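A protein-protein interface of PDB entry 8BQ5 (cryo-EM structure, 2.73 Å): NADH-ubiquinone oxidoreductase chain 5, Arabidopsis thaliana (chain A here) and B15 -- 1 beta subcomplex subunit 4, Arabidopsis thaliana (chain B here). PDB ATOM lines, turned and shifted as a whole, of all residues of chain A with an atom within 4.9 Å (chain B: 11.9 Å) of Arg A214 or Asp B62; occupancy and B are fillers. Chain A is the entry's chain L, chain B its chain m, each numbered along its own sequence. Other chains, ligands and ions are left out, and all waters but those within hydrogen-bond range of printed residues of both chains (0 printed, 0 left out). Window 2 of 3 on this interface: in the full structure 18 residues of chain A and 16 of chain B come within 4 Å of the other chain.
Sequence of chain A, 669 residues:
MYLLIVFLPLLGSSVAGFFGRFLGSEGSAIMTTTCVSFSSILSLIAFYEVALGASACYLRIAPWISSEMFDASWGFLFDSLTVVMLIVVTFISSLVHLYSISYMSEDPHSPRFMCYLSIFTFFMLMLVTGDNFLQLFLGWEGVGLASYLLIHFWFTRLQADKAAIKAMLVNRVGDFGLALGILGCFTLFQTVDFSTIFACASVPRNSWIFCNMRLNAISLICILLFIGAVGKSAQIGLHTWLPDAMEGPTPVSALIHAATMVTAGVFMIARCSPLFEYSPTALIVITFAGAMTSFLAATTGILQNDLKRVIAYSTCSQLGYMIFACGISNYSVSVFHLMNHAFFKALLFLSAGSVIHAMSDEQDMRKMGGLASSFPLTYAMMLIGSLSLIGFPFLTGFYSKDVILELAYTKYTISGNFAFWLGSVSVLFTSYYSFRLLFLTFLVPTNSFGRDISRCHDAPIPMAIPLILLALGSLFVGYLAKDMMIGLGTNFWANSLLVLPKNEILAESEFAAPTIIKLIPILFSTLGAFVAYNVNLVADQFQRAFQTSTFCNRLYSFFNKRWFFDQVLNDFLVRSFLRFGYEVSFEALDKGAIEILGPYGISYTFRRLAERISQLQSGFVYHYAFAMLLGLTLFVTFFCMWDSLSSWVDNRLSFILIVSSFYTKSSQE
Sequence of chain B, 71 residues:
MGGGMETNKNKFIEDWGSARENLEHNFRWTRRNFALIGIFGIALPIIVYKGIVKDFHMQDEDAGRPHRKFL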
ATOM      1  N   SER A 207       4.113  24.812 -28.550  1.00  0.00           N
ATOM      2  CA  SER A 207       2.883  24.187 -29.009  1.00  0.00           C
ATOM      3  C   SER A 207       2.030  23.776 -27.815  1.00  0.00           C
ATOM      4  O   SER A 207       2.536  23.438 -26.743  1.00  0.00           O
ATOM      5  CB  SER A 207       3.188  22.969 -29.880  1.00  0.00           C
ATOM      6  OG  SER A 207       2.111  22.685 -30.756  1.00  0.00           O
ATOM      7  N   TRP A 208       0.714  23.757 -28.009  1.00  0.00           N
ATOM      8  CA  TRP A 208      -0.201  23.465 -26.880  1.00  0.00           C
ATOM      9  C   TRP A 208      -1.221  22.386 -27.252  1.00  0.00           C
ATOM     10  O   TRP A 208      -1.594  22.309 -28.435  1.00  0.00           O
ATOM     11  CB  TRP A 208      -0.913  24.757 -26.472  1.00  0.00           C
ATOM     12  CG  TRP A 208      -0.263  25.504 -25.355  1.00  0.00           C
ATOM     13  CD1 TRP A 208       0.889  25.189 -24.697  1.00  0.00           C
ATOM     14  CD2 TRP A 208      -0.758  26.706 -24.748  1.00  0.00           C
ATOM     15  NE1 TRP A 208       1.148  26.117 -23.725  1.00  0.00           N
ATOM     16  CE2 TRP A 208       0.155  27.059 -23.734  1.00  0.00           C
ATOM     17  CE3 TRP A 208      -1.880  27.512 -24.965  1.00  0.00           C
ATOM     18  CZ2 TRP A 208      -0.024  28.187 -22.940  1.00  0.00           C
ATOM     19  CZ3 TRP A 208      -2.054  28.629 -24.182  1.00  0.00           C
ATOM     20  CH2 TRP A 208      -1.137  28.956 -23.186  1.00  0.00           C
ATOM     21  N   ILE A 209      -1.665  21.596 -26.274  1.00  0.00           N
ATOM     22  CA  ILE A 209      -2.752  20.606 -26.544  1.00  0.00           C
ATOM     23  C   ILE A 209      -4.097  21.303 -26.326  1.00  0.00           C
ATOM     24  O   ILE A 209      -4.368  21.704 -25.183  1.00  0.00           O
ATOM     25  CB  ILE A 209      -2.597  19.342 -25.675  1.00  0.00           C
ATOM     26  CG1 ILE A 209      -1.198  18.741 -25.808  1.00  0.00           C
ATOM     27  CG2 ILE A 209      -3.668  18.326 -26.028  1.00  0.00           C
ATOM     28  CD1 ILE A 209      -0.896  18.269 -27.205  1.00  0.00           C
ATOM     29  N   ASN A 212      -7.773  18.010 -27.811  1.00  0.00           N
ATOM     30  CA  ASN A 212      -7.005  16.785 -28.159  1.00  0.00           C
ATOM     31  C   ASN A 212      -6.232  17.048 -29.454  1.00  0.00           C
ATOM     32  O   ASN A 212      -6.174  16.140 -30.299  1.00  0.00           O
ATOM     33  CB  ASN A 212      -7.903  15.545 -28.224  1.00  0.00           C
ATOM     34  CG  ASN A 212      -8.695  15.353 -26.953  1.00  0.00           C
ATOM     35  OD1 ASN A 212      -8.259  15.771 -25.883  1.00  0.00           O
ATOM     36  ND2 ASN A 212      -9.857  14.735 -27.062  1.00  0.00           N
ATOM     37  N   MET A 213      -5.653  18.244 -29.585  1.00  0.00           N
ATOM     38  CA  MET A 213      -4.926  18.620 -30.825  1.00  0.00           C
ATOM     39  C   MET A 213      -3.699  19.459 -30.478  1.00  0.00           C
ATOM     40  O   MET A 213      -3.747  20.167 -29.470  1.00  0.00           O
ATOM     41  CB  MET A 213      -5.817  19.452 -31.749  1.00  0.00           C
ATOM     42  CG  MET A 213      -6.765  18.649 -32.610  1.00  0.00           C
ATOM     43  SD  MET A 213      -7.527  19.709 -33.864  1.00  0.00           S
ATOM     44  CE  MET A 213      -8.260  20.972 -32.827  1.00  0.00           C
ATOM     45  N   ARG A 214      -2.662  19.401 -31.309  1.00  0.00           N
ATOM     46  CA  ARG A 214      -1.445  20.178 -31.118  1.00  0.00           C
ATOM     47  C   ARG A 214      -1.552  21.453 -31.946  1.00  0.00           C
ATOM     48  O   ARG A 214      -1.608  21.393 -33.178  1.00  0.00           O
ATOM     49  CB  ARG A 214      -0.210  19.370 -31.520  1.00  0.00           C
ATOM     50  CG  ARG A 214       0.589  18.841 -30.340  1.00  0.00           C
ATOM     51  CD  ARG A 214       1.488  17.677 -30.726  1.00  0.00           C
ATOM     52  NE  ARG A 214       0.753  16.422 -30.821  1.00  0.00           N
ATOM     53  CZ  ARG A 214       0.845  15.429 -29.947  1.00  0.00           C
ATOM     54  NH1 ARG A 214       1.626  15.515 -28.882  1.00  0.00           N
ATOM     55  NH2 ARG A 214       0.135  14.323 -30.144  1.00  0.00           N
ATOM     56  N   LEU A 215      -1.589  22.600 -31.270  1.00  0.00           N
ATOM     57  CA  LEU A 215      -1.735  23.890 -31.929  1.00  0.00           C
ATOM     58  C   LEU A 215      -0.718  24.881 -31.380  1.00  0.00           C
ATOM     59  O   LEU A 215      -0.251  24.765 -30.244  1.00  0.00           O
ATOM     60  CB  LEU A 215      -3.146  24.477 -31.757  1.00  0.00           C
ATOM     61  CG  LEU A 215      -4.369  23.562 -31.815  1.00  0.00           C
ATOM     62  CD1 LEU A 215      -5.599  24.308 -31.334  1.00  0.00           C
ATOM     63  CD2 LEU A 215      -4.578  23.069 -33.229  1.00  0.00           C
ATOM     64  N   ASN A 216      -0.391  25.866 -32.210  1.00  0.00           N
ATOM     65  CA  ASN A 216       0.491  26.946 -31.793  1.00  0.00           C
ATOM     66  C   ASN A 216      -0.218  27.839 -30.781  1.00  0.00           C
ATOM     67  O   ASN A 216      -1.356  28.262 -31.004  1.00  0.00           O
ATOM     68  CB  ASN A 216       0.934  27.754 -33.011  1.00  0.00           C
ATOM     69  CG  ASN A 216       1.592  29.059 -32.635  1.00  0.00           C
ATOM     70  OD1 ASN A 216       1.029  30.131 -32.845  1.00  0.00           O
ATOM     71  ND2 ASN A 216       2.796  28.978 -32.084  1.00  0.00           N
ATOM     72  N   GLY B  51     -11.412  11.622 -24.014  1.00  0.00           N
ATOM     73  CA  GLY B  51     -10.837  12.870 -24.489  1.00  0.00           C
ATOM     74  C   GLY B  51     -10.043  13.584 -23.414  1.00  0.00           C
ATOM     75  O   GLY B  51      -9.019  14.210 -23.691  1.00  0.00           O
ATOM     76  N   VAL B  53      -8.565  12.035 -20.772  1.00  0.00           N
ATOM     77  CA  VAL B  53      -7.370  11.231 -20.531  1.00  0.00           C
ATOM     78  C   VAL B  53      -6.358  11.423 -21.655  1.00  0.00           C
ATOM     79  O   VAL B  53      -5.154  11.564 -21.407  1.00  0.00           O
ATOM     80  CB  VAL B  53      -7.750   9.749 -20.356  1.00  0.00           C
ATOM     81  CG1 VAL B  53      -6.521   8.863 -20.482  1.00  0.00           C
ATOM     82  CG2 VAL B  53      -8.416   9.531 -19.014  1.00  0.00           C
ATOM     83  N   LYS B  54      -6.828  11.433 -22.904  1.00  0.00           N
ATOM     84  CA  LYS B  54      -5.925  11.629 -24.034  1.00  0.00           C
ATOM     85  C   LYS B  54      -5.266  13.001 -23.971  1.00  0.00           C
ATOM     86  O   LYS B  54      -4.111  13.166 -24.380  1.00  0.00           O
ATOM     87  CB  LYS B  54      -6.693  11.446 -25.344  1.00  0.00           C
ATOM     88  CG  LYS B  54      -6.075  12.124 -26.552  1.00  0.00           C
ATOM     89  CD  LYS B  54      -5.076  11.201 -27.225  1.00  0.00           C
ATOM     90  CE  LYS B  54      -5.788  10.146 -28.054  1.00  0.00           C
ATOM     91  NZ  LYS B  54      -4.968   8.916 -28.221  1.00  0.00           N
ATOM     92  N   ASP B  55      -5.981  13.991 -23.433  1.00  0.00           N
ATOM     93  CA  ASP B  55      -5.417  15.326 -23.268  1.00  0.00           C
ATOM     94  C   ASP B  55      -4.211  15.291 -22.334  1.00  0.00           C
ATOM     95  O   ASP B  55      -3.198  15.954 -22.580  1.00  0.00           O
ATOM     96  CB  ASP B  55      -6.494  16.273 -22.733  1.00  0.00           C
ATOM     97  CG  ASP B  55      -6.112  17.732 -22.863  1.00  0.00           C
ATOM     98  OD1 ASP B  55      -6.088  18.238 -24.004  1.00  0.00           O
ATOM     99  OD2 ASP B  55      -5.831  18.374 -21.834  1.00  0.00           O
ATOM    100  N   PHE B  56      -4.309  14.518 -21.248  1.00  0.00           N
ATOM    101  CA  PHE B  56      -3.162  14.327 -20.366  1.00  0.00           C
ATOM    102  C   PHE B  56      -2.039  13.578 -21.070  1.00  0.00           C
ATOM    103  O   PHE B  56      -0.867  13.961 -20.965  1.00  0.00           O
ATOM    104  CB  PHE B  56      -3.578  13.569 -19.104  1.00  0.00           C
ATOM    105  CG  PHE B  56      -4.351  14.394 -18.116  1.00  0.00           C
ATOM    106  CD1 PHE B  56      -3.821  15.567 -17.603  1.00  0.00           C
ATOM    107  CD2 PHE B  56      -5.597  13.980 -17.678  1.00  0.00           C
ATOM    108  CE1 PHE B  56      -4.530  16.319 -16.685  1.00  0.00           C
ATOM    109  CE2 PHE B  56      -6.309  14.728 -16.761  1.00  0.00           C
ATOM    110  CZ  PHE B  56      -5.774  15.898 -16.264  1.00  0.00           C
ATOM    111  N   HIS B  57      -2.375  12.503 -21.789  1.00  0.00           N
ATOM    112  CA  HIS B  57      -1.350  11.691 -22.437  1.00  0.00           C
ATOM    113  C   HIS B  57      -0.581  12.497 -23.474  1.00  0.00           C
ATOM    114  O   HIS B  57       0.637  12.337 -23.615  1.00  0.00           O
ATOM    115  CB  HIS B  57      -1.979  10.461 -23.089  1.00  0.00           C
ATOM    116  CG  HIS B  57      -2.404   9.407 -22.117  1.00  0.00           C
ATOM    117  ND1 HIS B  57      -3.124   8.295 -22.494  1.00  0.00           N
ATOM    118  CD2 HIS B  57      -2.222   9.302 -20.780  1.00  0.00           C
ATOM    119  CE1 HIS B  57      -3.360   7.545 -21.433  1.00  0.00           C
ATOM    120  NE2 HIS B  57      -2.826   8.134 -20.379  1.00  0.00           N
ATOM    121  N   MET B  58      -1.276  13.356 -24.217  1.00  0.00           N
ATOM    122  CA  MET B  58      -0.597  14.211 -25.180  1.00  0.00           C
ATOM    123  C   MET B  58       0.335  15.190 -24.477  1.00  0.00           C
ATOM    124  O   MET B  58       1.417  15.503 -24.988  1.00  0.00           O
ATOM    125  CB  MET B  58      -1.628  14.941 -26.039  1.00  0.00           C
ATOM    126  CG  MET B  58      -2.304  14.028 -27.052  1.00  0.00           C
ATOM    127  SD  MET B  58      -3.730  14.760 -27.872  1.00  0.00           S
ATOM    128  CE  MET B  58      -2.927  15.829 -29.056  1.00  0.00           C
ATOM    129  N   GLN B  59      -0.064  15.680 -23.301  1.00  0.00           N
ATOM    130  CA  GLN B  59       0.840  16.491 -22.495  1.00  0.00           C
ATOM    131  C   GLN B  59       2.032  15.673 -22.017  1.00  0.00           C
ATOM    132  O   GLN B  59       3.127  16.212 -21.815  1.00  0.00           O
ATOM    133  CB  GLN B  59       0.093  17.084 -21.301  1.00  0.00           C
ATOM    134  CG  GLN B  59      -0.735  18.310 -21.623  1.00  0.00           C
ATOM    135  CD  GLN B  59      -1.429  18.872 -20.398  1.00  0.00           C
ATOM    136  OE1 GLN B  59      -0.986  19.865 -19.822  1.00  0.00           O
ATOM    137  NE2 GLN B  59      -2.520  18.232 -19.989  1.00  0.00           N
ATOM    138  N   ASP B  60       1.831  14.369 -21.807  1.00  0.00           N
ATOM    139  CA  ASP B  60       2.925  13.510 -21.364  1.00  0.00           C
ATOM    140  C   ASP B  60       3.988  13.368 -22.448  1.00  0.00           C
ATOM    141  O   ASP B  60       5.180  13.573 -22.194  1.00  0.00           O
ATOM    142  CB  ASP B  60       2.378  12.143 -20.954  1.00  0.00           C
ATOM    143  CG  ASP B  60       2.163  12.029 -19.458  1.00  0.00           C
ATOM    144  OD1 ASP B  60       2.664  12.903 -18.722  1.00  0.00           O
ATOM    145  OD2 ASP B  60       1.490  11.073 -19.019  1.00  0.00           O
ATOM    146  N   GLU B  61       3.572  13.025 -23.670  1.00  0.00           N
ATOM    147  CA  GLU B  61       4.529  12.881 -24.761  1.00  0.00           C
ATOM    148  C   GLU B  61       5.100  14.219 -25.210  1.00  0.00           C
ATOM    149  O   GLU B  61       6.249  14.266 -25.663  1.00  0.00           O
ATOM    150  CB  GLU B  61       3.882  12.169 -25.949  1.00  0.00           C
ATOM    151  CG  GLU B  61       2.544  12.739 -26.367  1.00  0.00           C
ATOM    152  CD  GLU B  61       1.645  11.698 -27.001  1.00  0.00           C
ATOM    153  OE1 GLU B  61       1.999  11.198 -28.087  1.00  0.00           O
ATOM    154  OE2 GLU B  61       0.587  11.381 -26.418  1.00  0.00           O
ATOM    155  N   ASP B  62       4.326  15.301 -25.107  1.00  0.00           N
ATOM    156  CA  ASP B  62       4.854  16.629 -25.397  1.00  0.00           C
ATOM    157  C   ASP B  62       5.983  17.012 -24.453  1.00  0.00           C
ATOM    158  O   ASP B  62       6.849  17.809 -24.832  1.00  0.00           O
ATOM    159  CB  ASP B  62       3.734  17.667 -25.309  1.00  0.00           C
ATOM    160  CG  ASP B  62       2.992  17.840 -26.620  1.00  0.00           C
ATOM    161  OD1 ASP B  62       3.203  17.028 -27.545  1.00  0.00           O
ATOM    162  OD2 ASP B  62       2.182  18.786 -26.718  1.00  0.00           O
ATOM    163  N   ALA B  63       5.989  16.470 -23.237  1.00  0.00           N
ATOM    164  CA  ALA B  63       7.021  16.740 -22.246  1.00  0.00           C
ATOM    165  C   ALA B  63       8.023  15.602 -22.116  1.00  0.00           C
ATOM    166  O   ALA B  63       8.792  15.576 -21.149  1.00  0.00           O
ATOM    167  CB  ALA B  63       6.382  17.029 -20.886  1.00  0.00           C
ATOM    168  N   GLY B  64       8.024  14.658 -23.053  1.00  0.00           N
ATOM    169  CA  GLY B  64       8.977  13.558 -23.012  1.00  0.00           C
ATOM    170  C   GLY B  64       8.853  12.667 -21.796  1.00  0.00           C
ATOM    171  O   GLY B  64       9.871  12.288 -21.201  1.00  0.00           O
ATOM    172  N   ARG B  65       7.630  12.321 -21.411  1.00  0.00           N
ATOM    173  CA  ARG B  65       7.372  11.487 -20.249  1.00  0.00           C
ATOM    174  C   ARG B  65       6.391  10.383 -20.609  1.00  0.00           C
ATOM    175  O   ARG B  65       5.506  10.582 -21.447  1.00  0.00           O
ATOM    176  CB  ARG B  65       6.807  12.320 -19.090  1.00  0.00           C
ATOM    177  CG  ARG B  65       7.858  12.809 -18.107  1.00  0.00           C
ATOM    178  CD  ARG B  65       7.239  13.522 -16.910  1.00  0.00           C
ATOM    179  NE  ARG B  65       6.591  14.773 -17.288  1.00  0.00           N
ATOM    180  CZ  ARG B  65       5.302  14.901 -17.577  1.00  0.00           C
ATOM    181  NH1 ARG B  65       4.473  13.872 -17.507  1.00  0.00           N
ATOM    182  NH2 ARG B  65       4.834  16.091 -17.940  1.00  0.00           N
ATOM    183  N   PRO B  66       6.521   9.212 -19.990  1.00  0.00           N
ATOM    184  CA  PRO B  66       5.610   8.103 -20.296  1.00  0.00           C
ATOM    185  C   PRO B  66       4.182   8.433 -19.889  1.00  0.00           C
ATOM    186  O   PRO B  66       3.922   9.267 -19.020  1.00  0.00           O
ATOM    187  CB  PRO B  66       6.171   6.934 -19.481  1.00  0.00           C
ATOM    188  CG  PRO B  66       7.571   7.333 -19.129  1.00  0.00           C
ATOM    189  CD  PRO B  66       7.566   8.822 -19.028  1.00  0.00           C
ATOM    190  N   HIS B  67       3.245   7.756 -20.551  1.00  0.00           N
ATOM    191  CA  HIS B  67       1.827   8.020 -20.343  1.00  0.00           C
ATOM    192  C   HIS B  67       1.443   7.787 -18.887  1.00  0.00           C
ATOM    193  O   HIS B  67       1.900   6.829 -18.257  1.00  0.00           O
ATOM    194  CB  HIS B  67       0.985   7.132 -21.258  1.00  0.00           C
ATOM    195  CG  HIS B  67       0.776   7.700 -22.627  1.00  0.00           C
ATOM    196  ND1 HIS B  67      -0.189   7.226 -23.489  1.00  0.00           N
ATOM    197  CD2 HIS B  67       1.408   8.699 -23.286  1.00  0.00           C
ATOM    198  CE1 HIS B  67      -0.142   7.907 -24.619  1.00  0.00           C
ATOM    199  NE2 HIS B  67       0.818   8.809 -24.521  1.00  0.00           N
ATOM    200  N   ARG B  68       0.601   8.669 -18.356  1.00  0.00           N
ATOM    201  CA  ARG B  68       0.174   8.554 -16.970  1.00  0.00           C
ATOM    202  C   ARG B  68      -0.938   7.523 -16.843  1.00  0.00           C
ATOM    203  O   ARG B  68      -1.947   7.588 -17.551  1.00  0.00           O
ATOM    204  CB  ARG B  68      -0.301   9.908 -16.445  1.00  0.00           C
ATOM    205  CG  ARG B  68       0.315  10.305 -15.114  1.00  0.00           C
ATOM    206  CD  ARG B  68      -0.038  11.734 -14.723  1.00  0.00           C
ATOM    207  NE  ARG B  68       0.350  12.700 -15.745  1.00  0.00           N
ATOM    208  CZ  ARG B  68      -0.481  13.556 -16.322  1.00  0.00           C
ATOM    209  NH1 ARG B  68      -1.754  13.625 -15.972  1.00  0.00           N
ATOM    210  NH2 ARG B  68      -0.021  14.368 -17.270  1.00  0.00           N
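Among the printed residues, merely in contact across the chains: Ile A209 with Asp B55 (3.2 Å), Ile A209 with Asp B62 (3.2 Å), Arg A214 with Met B58 (3.6 Å), Ile A209 with Met B58 (3.6 Å), Asn A212 with Asp B55 (3.6 Å), Met A213 with Met B58 (3.7 Å) and Arg A214 with Glu B61 (3.9 Å).
The side-chain carboxylate (OE2) of Glu B61 sits at hydrogen-bond distance from a ring nitrogen (NE2) of His B67 (3.2 Å). The backbone NH (N) of Met B58 lies close to the side-chain carboxylate (OE2) of Glu B61, 3.5 Å away.
Of the printed residues of chain B, Arg A214 touches Met B58, Glu B61 and Asp B62. Of the printed residues of chain A, Asp B62 touches Ile A209 (3.2 Å) and Arg A214 (2.6 Å). No residue of chain B comes within 4 Å of Ser A207. Of chain B, only Asp B55 (3.2 Å), Met B58 (3.6 Å) and Asp B62 (3.2 Å) come within 4 Å of Ile A209. No residue of chain B comes within 4 Å of Leu A215. Of the printed residues of chain A, Met B58 touches Ile A209 (3.6 Å), Asn A212 (3.5 Å), Met A213 (3.7 Å) and Arg A214 (3.6 Å). Of the printed residues of chain A, Gly B51 touches Asn A212. Printed residues of chain A within 4 Å of Asp B55: Ile A209 (3.2 Å) and Asn A212 (3.6 Å). Of the printed residues of chain A, Glu B61 touches Arg A214 (3.9 Å). Printed residues of chain B within 4 Å of Asn A212: Gly B51 (2.8 Å), Asp B55 (3.6 Å) and Met B58 (3.5 Å). Gly B64 touches none of the printed residues of chain A. The nearest residue of chain B that does not touch Arg A214 is Gln B59 (5.8 Å). The nearest residue of chain A that does not touch Asp B62 is Ser A207 (4.7 Å).
Printed residues of chain B that touch a printed residue of chain A: Gly B51, Asp B55, Met B58, Glu B61 and Asp B62. Of the 8 printed residues of chain A, 4 touch a printed residue of chain B. Hydrophobic or aromatic side chains of chain A within 4 Å of the printed part of chain B: Ile A209. Along chain A the printed residues that touch a printed residue of chain B span positions 209 to 214.
OD1 of Asn A212 sits close to O of Gly B51, at 2.8 Å. The backbone carbonyl oxygen (O) of Asn A212 sits close to the side-chain sulfur (SD) of Met B58 (3.7 Å). OD1 of Asp B62 is in salt-bridge range of NH1 of Arg A214 (2.6 Å).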
